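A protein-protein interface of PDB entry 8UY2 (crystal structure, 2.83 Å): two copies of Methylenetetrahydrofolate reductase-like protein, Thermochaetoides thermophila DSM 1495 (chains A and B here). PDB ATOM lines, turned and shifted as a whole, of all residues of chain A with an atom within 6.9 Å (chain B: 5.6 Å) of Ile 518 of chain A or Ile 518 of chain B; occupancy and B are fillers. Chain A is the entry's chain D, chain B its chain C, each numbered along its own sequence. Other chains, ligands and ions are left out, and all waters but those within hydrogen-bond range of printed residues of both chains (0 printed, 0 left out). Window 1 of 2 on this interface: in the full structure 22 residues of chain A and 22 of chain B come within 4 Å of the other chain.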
ATOM      1  N   LYS A 460      14.760 -16.103  15.747  1.00  0.00           N
ATOM      2  CA  LYS A 460      14.843 -14.806  15.103  1.00  0.00           C
ATOM      3  C   LYS A 460      14.122 -13.821  16.000  1.00  0.00           C
ATOM      4  O   LYS A 460      13.021 -14.124  16.445  1.00  0.00           O
ATOM      5  CB  LYS A 460      14.247 -14.816  13.691  1.00  0.00           C
ATOM      6  CG  LYS A 460      15.074 -15.581  12.678  1.00  0.00           C
ATOM      7  CD  LYS A 460      14.319 -15.837  11.391  1.00  0.00           C
ATOM      8  CE  LYS A 460      15.077 -16.605  10.360  1.00  0.00           C
ATOM      9  NZ  LYS A 460      14.196 -17.120   9.308  1.00  0.00           N
ATOM     10  N   PRO A 505       5.796 -19.303   4.446  1.00  0.00           N
ATOM     11  CA  PRO A 505       6.113 -19.242   5.873  1.00  0.00           C
ATOM     12  C   PRO A 505       7.580 -18.900   6.153  1.00  0.00           C
ATOM     13  O   PRO A 505       8.462 -19.328   5.402  1.00  0.00           O
ATOM     14  CB  PRO A 505       5.736 -20.632   6.382  1.00  0.00           C
ATOM     15  CG  PRO A 505       5.829 -21.519   5.196  1.00  0.00           C
ATOM     16  CD  PRO A 505       5.460 -20.661   4.021  1.00  0.00           C
ATOM     17  N   ASN A 506       7.808 -18.101   7.212  1.00  0.00           N
ATOM     18  CA  ASN A 506       9.131 -17.772   7.707  1.00  0.00           C
ATOM     19  C   ASN A 506       9.261 -18.336   9.115  1.00  0.00           C
ATOM     20  O   ASN A 506       8.532 -17.906  10.000  1.00  0.00           O
ATOM     21  CB  ASN A 506       9.354 -16.272   7.671  1.00  0.00           C
ATOM     22  CG  ASN A 506      10.753 -15.819   8.077  1.00  0.00           C
ATOM     23  OD1 ASN A 506      11.690 -16.618   8.199  1.00  0.00           O
ATOM     24  ND2 ASN A 506      10.939 -14.521   8.233  1.00  0.00           N
ATOM     25  N   ALA A 507      10.216 -19.254   9.326  1.00  0.00           N
ATOM     26  CA  ALA A 507      10.462 -19.834  10.645  1.00  0.00           C
ATOM     27  C   ALA A 507      11.202 -18.822  11.513  1.00  0.00           C
ATOM     28  O   ALA A 507      12.226 -18.313  11.080  1.00  0.00           O
ATOM     29  CB  ALA A 507      11.224 -21.126  10.519  1.00  0.00           C
ATOM     30  N   VAL A 508      10.671 -18.530  12.700  1.00  0.00           N
ATOM     31  CA  VAL A 508      11.288 -17.586  13.637  1.00  0.00           C
ATOM     32  C   VAL A 508      11.669 -18.227  14.968  1.00  0.00           C
ATOM     33  O   VAL A 508      12.306 -17.568  15.782  1.00  0.00           O
ATOM     34  CB  VAL A 508      10.362 -16.387  13.848  1.00  0.00           C
ATOM     35  CG1 VAL A 508       9.969 -15.764  12.513  1.00  0.00           C
ATOM     36  CG2 VAL A 508       9.095 -16.719  14.636  1.00  0.00           C
ATOM     37  N   THR A 509      11.212 -19.461  15.237  1.00  0.00           N
ATOM     38  CA  THR A 509      11.740 -20.273  16.313  1.00  0.00           C
ATOM     39  C   THR A 509      11.928 -21.682  15.769  1.00  0.00           C
ATOM     40  O   THR A 509      10.999 -22.236  15.181  1.00  0.00           O
ATOM     41  CB  THR A 509      10.802 -20.283  17.511  1.00  0.00           C
ATOM     42  OG1 THR A 509      10.537 -18.960  17.955  1.00  0.00           O
ATOM     43  CG2 THR A 509      11.356 -21.052  18.690  1.00  0.00           C
ATOM     44  N   TRP A 510      13.121 -22.254  15.965  1.00  0.00           N
ATOM     45  CA  TRP A 510      13.340 -23.639  15.615  1.00  0.00           C
ATOM     46  C   TRP A 510      14.274 -24.324  16.594  1.00  0.00           C
ATOM     47  O   TRP A 510      14.916 -23.667  17.404  1.00  0.00           O
ATOM     48  CB  TRP A 510      13.795 -23.764  14.158  1.00  0.00           C
ATOM     49  CG  TRP A 510      15.129 -23.156  13.877  1.00  0.00           C
ATOM     50  CD1 TRP A 510      16.327 -23.785  13.761  1.00  0.00           C
ATOM     51  CD2 TRP A 510      15.385 -21.764  13.660  1.00  0.00           C
ATOM     52  NE1 TRP A 510      17.318 -22.869  13.498  1.00  0.00           N
ATOM     53  CE2 TRP A 510      16.769 -21.627  13.399  1.00  0.00           C
ATOM     54  CE3 TRP A 510      14.571 -20.620  13.636  1.00  0.00           C
ATOM     55  CZ2 TRP A 510      17.355 -20.387  13.169  1.00  0.00           C
ATOM     56  CZ3 TRP A 510      15.151 -19.399  13.379  1.00  0.00           C
ATOM     57  CH2 TRP A 510      16.522 -19.289  13.157  1.00  0.00           C
ATOM     58  N   GLY A 511      14.308 -25.661  16.522  1.00  0.00           N
ATOM     59  CA  GLY A 511      15.039 -26.482  17.469  1.00  0.00           C
ATOM     60  C   GLY A 511      15.661 -27.698  16.800  1.00  0.00           C
ATOM     61  O   GLY A 511      15.006 -28.349  15.975  1.00  0.00           O
ATOM     62  N   VAL A 512      16.896 -28.018  17.210  1.00  0.00           N
ATOM     63  CA  VAL A 512      17.665 -29.128  16.675  1.00  0.00           C
ATOM     64  C   VAL A 512      17.805 -30.134  17.808  1.00  0.00           C
ATOM     65  O   VAL A 512      18.483 -29.830  18.787  1.00  0.00           O
ATOM     66  CB  VAL A 512      19.024 -28.668  16.143  1.00  0.00           C
ATOM     67  CG1 VAL A 512      19.741 -29.788  15.397  1.00  0.00           C
ATOM     68  CG2 VAL A 512      18.865 -27.449  15.240  1.00  0.00           C
ATOM     69  N   PHE A 513      17.188 -31.318  17.648  1.00  0.00           N
ATOM     70  CA  PHE A 513      17.163 -32.325  18.684  1.00  0.00           C
ATOM     71  C   PHE A 513      17.703 -33.649  18.157  1.00  0.00           C
ATOM     72  O   PHE A 513      17.481 -33.967  16.981  1.00  0.00           O
ATOM     73  CB  PHE A 513      15.760 -32.491  19.218  1.00  0.00           C
ATOM     74  CG  PHE A 513      15.174 -31.204  19.742  1.00  0.00           C
ATOM     75  CD1 PHE A 513      15.526 -30.717  21.002  1.00  0.00           C
ATOM     76  CD2 PHE A 513      14.263 -30.492  18.969  1.00  0.00           C
ATOM     77  CE1 PHE A 513      14.969 -29.539  21.486  1.00  0.00           C
ATOM     78  CE2 PHE A 513      13.707 -29.310  19.454  1.00  0.00           C
ATOM     79  CZ  PHE A 513      14.066 -28.831  20.716  1.00  0.00           C
ATOM     80  N   LYS A 516      16.157 -36.293  15.226  1.00  0.00           N
ATOM     81  CA  LYS A 516      14.913 -35.701  14.763  1.00  0.00           C
ATOM     82  C   LYS A 516      15.141 -34.730  13.608  1.00  0.00           C
ATOM     83  O   LYS A 516      16.256 -34.239  13.397  1.00  0.00           O
ATOM     84  CB  LYS A 516      14.184 -35.097  15.957  1.00  0.00           C
ATOM     85  CG  LYS A 516      13.534 -36.213  16.799  1.00  0.00           C
ATOM     86  CD  LYS A 516      12.828 -35.795  18.091  1.00  0.00           C
ATOM     87  CE  LYS A 516      11.624 -34.894  17.951  1.00  0.00           C
ATOM     88  NZ  LYS A 516      11.041 -34.464  19.236  1.00  0.00           N
ATOM     89  N   GLU A 517      14.062 -34.486  12.845  1.00  0.00           N
ATOM     90  CA  GLU A 517      13.977 -33.381  11.907  1.00  0.00           C
ATOM     91  C   GLU A 517      13.842 -32.082  12.689  1.00  0.00           C
ATOM     92  O   GLU A 517      13.423 -32.094  13.847  1.00  0.00           O
ATOM     93  CB  GLU A 517      12.830 -33.548  10.902  1.00  0.00           C
ATOM     94  CG  GLU A 517      13.217 -34.338   9.651  1.00  0.00           C
ATOM     95  CD  GLU A 517      12.287 -34.156   8.444  1.00  0.00           C
ATOM     96  OE1 GLU A 517      11.107 -34.556   8.582  1.00  0.00           O
ATOM     97  OE2 GLU A 517      12.705 -33.598   7.381  1.00  0.00           O
ATOM     98  N   ILE A 518      14.148 -30.980  12.009  1.00  0.00           N
ATOM     99  CA  ILE A 518      14.141 -29.673  12.633  1.00  0.00           C
ATOM    100  C   ILE A 518      12.700 -29.312  12.991  1.00  0.00           C
ATOM    101  O   ILE A 518      11.841 -29.330  12.119  1.00  0.00           O
ATOM    102  CB  ILE A 518      14.770 -28.619  11.716  1.00  0.00           C
ATOM    103  CG1 ILE A 518      16.162 -29.016  11.229  1.00  0.00           C
ATOM    104  CG2 ILE A 518      14.777 -27.254  12.408  1.00  0.00           C
ATOM    105  CD1 ILE A 518      17.204 -29.225  12.315  1.00  0.00           C
ATOM    106  N   VAL A 519      12.479 -28.942  14.257  1.00  0.00           N
ATOM    107  CA  VAL A 519      11.173 -28.565  14.768  1.00  0.00           C
ATOM    108  C   VAL A 519      11.028 -27.043  14.661  1.00  0.00           C
ATOM    109  O   VAL A 519      11.887 -26.305  15.114  1.00  0.00           O
ATOM    110  CB  VAL A 519      11.045 -29.069  16.210  1.00  0.00           C
ATOM    111  CG1 VAL A 519       9.744 -28.640  16.849  1.00  0.00           C
ATOM    112  CG2 VAL A 519      11.150 -30.589  16.274  1.00  0.00           C
ATOM    113  N   GLN A 520       9.880 -26.593  14.138  1.00  0.00           N
ATOM    114  CA  GLN A 520       9.634 -25.202  13.769  1.00  0.00           C
ATOM    115  C   GLN A 520       8.306 -24.750  14.356  1.00  0.00           C
ATOM    116  O   GLN A 520       7.367 -24.510  13.622  1.00  0.00           O
ATOM    117  CB  GLN A 520       9.611 -25.103  12.256  1.00  0.00           C
ATOM    118  CG  GLN A 520      10.894 -25.576  11.616  1.00  0.00           C
ATOM    119  CD  GLN A 520      10.847 -25.386  10.114  1.00  0.00           C
ATOM    120  OE1 GLN A 520      10.643 -24.260   9.632  1.00  0.00           O
ATOM    121  NE2 GLN A 520      11.066 -26.451   9.350  1.00  0.00           N
ATOM    122  N   PRO A 521       8.193 -24.599  15.693  1.00  0.00           N
ATOM    123  CA  PRO A 521       6.937 -24.212  16.315  1.00  0.00           C
ATOM    124  C   PRO A 521       6.407 -22.818  16.052  1.00  0.00           C
ATOM    125  O   PRO A 521       5.269 -22.559  16.384  1.00  0.00           O
ATOM    126  CB  PRO A 521       7.241 -24.433  17.797  1.00  0.00           C
ATOM    127  CG  PRO A 521       8.690 -24.233  17.932  1.00  0.00           C
ATOM    128  CD  PRO A 521       9.268 -24.785  16.682  1.00  0.00           C
ATOM    129  N   ILE A 523       6.105 -19.597  13.319  1.00  0.00           N
ATOM    130  CA  ILE A 523       6.095 -19.266  11.910  1.00  0.00           C
ATOM    131  C   ILE A 523       5.425 -17.906  11.794  1.00  0.00           C
ATOM    132  O   ILE A 523       4.436 -17.640  12.480  1.00  0.00           O
ATOM    133  CB  ILE A 523       5.304 -20.321  11.117  1.00  0.00           C
ATOM    134  CG1 ILE A 523       5.775 -21.741  11.365  1.00  0.00           C
ATOM    135  CG2 ILE A 523       5.290 -20.000   9.631  1.00  0.00           C
ATOM    136  CD1 ILE A 523       7.217 -21.984  10.988  1.00  0.00           C
ATOM    137  N   ALA B 507      17.623 -34.999  10.614  1.00  0.00           N
ATOM    138  CA  ALA B 507      18.201 -33.954   9.777  1.00  0.00           C
ATOM    139  C   ALA B 507      19.671 -33.789  10.127  1.00  0.00           C
ATOM    140  O   ALA B 507      19.975 -33.614  11.297  1.00  0.00           O
ATOM    141  CB  ALA B 507      17.466 -32.658   9.962  1.00  0.00           C
ATOM    142  N   TRP B 510      21.029 -28.630   7.478  1.00  0.00           N
ATOM    143  CA  TRP B 510      19.924 -27.702   7.348  1.00  0.00           C
ATOM    144  C   TRP B 510      20.402 -26.276   7.166  1.00  0.00           C
ATOM    145  O   TRP B 510      21.577 -25.992   7.341  1.00  0.00           O
ATOM    146  CB  TRP B 510      18.953 -27.853   8.520  1.00  0.00           C
ATOM    147  CG  TRP B 510      19.525 -27.472   9.855  1.00  0.00           C
ATOM    148  CD1 TRP B 510      19.360 -26.313  10.543  1.00  0.00           C
ATOM    149  CD2 TRP B 510      20.356 -28.305  10.671  1.00  0.00           C
ATOM    150  NE1 TRP B 510      20.041 -26.363  11.731  1.00  0.00           N
ATOM    151  CE2 TRP B 510      20.633 -27.577  11.853  1.00  0.00           C
ATOM    152  CE3 TRP B 510      20.872 -29.604  10.525  1.00  0.00           C
ATOM    153  CZ2 TRP B 510      21.457 -28.087  12.855  1.00  0.00           C
ATOM    154  CZ3 TRP B 510      21.641 -30.129  11.541  1.00  0.00           C
ATOM    155  CH2 TRP B 510      21.943 -29.372  12.681  1.00  0.00           C
ATOM    156  N   GLY B 511      19.475 -25.402   6.765  1.00  0.00           N
ATOM    157  CA  GLY B 511      19.793 -24.039   6.386  1.00  0.00           C
ATOM    158  C   GLY B 511      18.681 -23.083   6.794  1.00  0.00           C
ATOM    159  O   GLY B 511      17.499 -23.394   6.622  1.00  0.00           O
ATOM    160  N   VAL B 512      19.083 -21.895   7.274  1.00  0.00           N
ATOM    161  CA  VAL B 512      18.179 -20.853   7.735  1.00  0.00           C
ATOM    162  C   VAL B 512      18.336 -19.702   6.765  1.00  0.00           C
ATOM    163  O   VAL B 512      19.407 -19.127   6.716  1.00  0.00           O
ATOM    164  CB  VAL B 512      18.493 -20.438   9.173  1.00  0.00           C
ATOM    165  CG1 VAL B 512      17.428 -19.511   9.738  1.00  0.00           C
ATOM    166  CG2 VAL B 512      18.663 -21.649  10.076  1.00  0.00           C
ATOM    167  N   LYS B 516      11.988 -17.762   4.943  1.00  0.00           N
ATOM    168  CA  LYS B 516      11.769 -19.151   4.583  1.00  0.00           C
ATOM    169  C   LYS B 516      11.678 -20.031   5.824  1.00  0.00           C
ATOM    170  O   LYS B 516      12.131 -19.656   6.916  1.00  0.00           O
ATOM    171  CB  LYS B 516      12.822 -19.599   3.572  1.00  0.00           C
ATOM    172  CG  LYS B 516      12.502 -19.005   2.189  1.00  0.00           C
ATOM    173  CD  LYS B 516      13.376 -19.367   0.994  1.00  0.00           C
ATOM    174  CE  LYS B 516      13.535 -20.845   0.677  1.00  0.00           C
ATOM    175  NZ  LYS B 516      14.419 -21.131  -0.468  1.00  0.00           N
ATOM    176  N   GLU B 517      11.062 -21.217   5.629  1.00  0.00           N
ATOM    177  CA  GLU B 517      11.108 -22.310   6.577  1.00  0.00           C
ATOM    178  C   GLU B 517      12.507 -22.916   6.546  1.00  0.00           C
ATOM    179  O   GLU B 517      13.251 -22.728   5.598  1.00  0.00           O
ATOM    180  CB  GLU B 517      10.024 -23.361   6.313  1.00  0.00           C
ATOM    181  CG  GLU B 517       8.689 -22.993   6.958  1.00  0.00           C
ATOM    182  CD  GLU B 517       7.552 -24.007   6.826  1.00  0.00           C
ATOM    183  OE1 GLU B 517       7.219 -24.423   5.683  1.00  0.00           O
ATOM    184  OE2 GLU B 517       6.983 -24.363   7.884  1.00  0.00           O
ATOM    185  N   ILE B 518      12.831 -23.685   7.574  1.00  0.00           N
ATOM    186  CA  ILE B 518      14.110 -24.357   7.651  1.00  0.00           C
ATOM    187  C   ILE B 518      14.191 -25.414   6.551  1.00  0.00           C
ATOM    188  O   ILE B 518      13.324 -26.255   6.461  1.00  0.00           O
ATOM    189  CB  ILE B 518      14.328 -24.969   9.028  1.00  0.00           C
ATOM    190  CG1 ILE B 518      14.124 -23.938  10.178  1.00  0.00           C
ATOM    191  CG2 ILE B 518      15.716 -25.605   9.081  1.00  0.00           C
ATOM    192  CD1 ILE B 518      15.040 -22.732  10.149  1.00  0.00           C
ATOM    193  N   VAL B 519      15.247 -25.359   5.740  1.00  0.00           N
ATOM    194  CA  VAL B 519      15.471 -26.245   4.618  1.00  0.00           C
ATOM    195  C   VAL B 519      16.384 -27.373   5.095  1.00  0.00           C
ATOM    196  O   VAL B 519      17.426 -27.124   5.676  1.00  0.00           O
ATOM    197  CB  VAL B 519      16.074 -25.453   3.454  1.00  0.00           C
ATOM    198  CG1 VAL B 519      16.445 -26.354   2.290  1.00  0.00           C
ATOM    199  CG2 VAL B 519      15.111 -24.376   2.969  1.00  0.00           C
ATOM    200  N   GLN B 520      16.007 -28.618   4.757  1.00  0.00           N
ATOM    201  CA  GLN B 520      16.611 -29.834   5.299  1.00  0.00           C
ATOM    202  C   GLN B 520      16.962 -30.783   4.169  1.00  0.00           C
ATOM    203  O   GLN B 520      16.365 -31.835   4.058  1.00  0.00           O
ATOM    204  CB  GLN B 520      15.621 -30.475   6.257  1.00  0.00           C
ATOM    205  CG  GLN B 520      15.192 -29.537   7.364  1.00  0.00           C
ATOM    206  CD  GLN B 520      14.274 -30.219   8.338  1.00  0.00           C
ATOM    207  OE1 GLN B 520      14.681 -31.210   8.946  1.00  0.00           O
ATOM    208  NE2 GLN B 520      13.061 -29.704   8.524  1.00  0.00           N
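The backbone NH of Ala 507 of chain B lies within hydrogen-bond range of the backbone carbonyl oxygen of Lys 516 of chain A. The side-chain amide oxygen (OD1) of Asn 506 of chain A lies close to the backbone carbonyl oxygen (O) of Lys 516 of chain B, 3.3 Å away. The backbone carbonyl oxygen (O) of Lys 516 of chain B is in hydrogen-bond range of the backbone NH (N) of Ala 507 of chain A, 3.1 Å away. The backbone NH of Glu 517 of chain B sits at hydrogen-bond distance from the backbone carbonyl oxygen of Pro 505 of chain A (3.2 Å). OE1 of Gln 520 of chain A sits at hydrogen-bond distance from N of Ile 518 of chain B, at 3.1 Å. The side-chain carboxylate (OE2) of Glu 517 of chain A lies close to the side-chain amide oxygen (OE1) of Gln 520 of chain B (3.5 Å). OE1 of Gln 520 of chain B lies within hydrogen-bond range of N of Ile 518 of chain A, 3.1 Å away.
The side-chain amide oxygen (OD1) of Asn 506 of chain A is in hydrogen-bond range of the side-chain amino group (NZ) of Lys 460 of chain A (2.8 Å). The backbone carbonyl oxygen (O) of Ala 507 of chain A is in hydrogen-bond range of the side-chain amino group (NZ) of Lys 460 of chain A, at 2.9 Å. N of Lys 460 of chain A is in hydrogen-bond range of O of Val 508 of chain A, 2.9 Å away.
Among the printed residues, pairs that only touch across the chains: Lys 460 of chain A with Val 512 of chain B (3.8 Å), Pro 505 of chain A with Lys 516 of chain B (3.3 Å), Trp 510 of chain A with Val 512 of chain B (3.5 Å), Trp 510 of chain A with Ile 518 of chain B (3.7 Å), Val 512 of chain A with Trp 510 of chain B (3.5 Å), Ile 518 of chain A with Trp 510 of chain B (3.7 Å), Ile 518 of chain A with Ile 518 of chain B (3.8 Å), Gln 520 of chain A with Glu 517 of chain B (3.5 Å), Gln 520 of chain A with Gln 520 of chain B (3.9 Å) and Ile 523 of chain A with Glu 517 of chain B (3.9 Å).
Ile 518 of chain A touches three residues of chain B. Ile 518 of chain B touches three residues of chain A. Of the printed residues of chain A, Val 512 of chain B touches Lys 460 and Trp 510. Of the printed residues of chain B, Ile 523 of chain A touches Glu 517 (3.9 Å). Printed residues of chain B within 4 Å of Val 512 of chain A: Trp 510. Printed residues of chain B within 4 Å of Pro 505 of chain A: Lys 516 (3.3 Å) and Glu 517 (3.2 Å). The nearest residue of chain B that does not touch Ile 518 of chain A is Ala 507 of chain B (4.1 Å).
Of the 17 printed residues of chain A, 11 touch a printed residue of chain B. Hydrophobic or aromatic side chains of chain A that line the printed part of chain B: Pro 505, Ala 507, Trp 510, Val 512, Ile 518 and Ile 523. Of the 9 printed residues of chain B, 7 touch a printed residue of chain A. Printed residues of chain B that touch a printed residue of chain A: Ala 507, Trp 510, Val 512, Lys 516, Glu 517, Ile 518 and Gln 520. Among the printed residues, no Asp or Glu carboxylate lies within 4 Å of a Lys or Arg side-chain nitrogen of the other chain.
Ala 507 of chain A touches Lys 516 of chain B, and with the chains exchanged Lys 516 of chain A touches Ala 507 of chain B. Glu 517 of chain A touches Gln 520 of chain B, and with the chains exchanged Gln 520 of chain A touches Glu 517 of chain B. Ile 518 of chain A touches its own counterpart, Ile 518 of chain B. Ile 518 of chain A touches Gln 520 of chain B, and with the chains exchanged Gln 520 of chain A touches Ile 518 of chain B. Of the 17 pairs that touch across the chains among the printed residues, 12 have their exchanged pair printed and touching as well.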
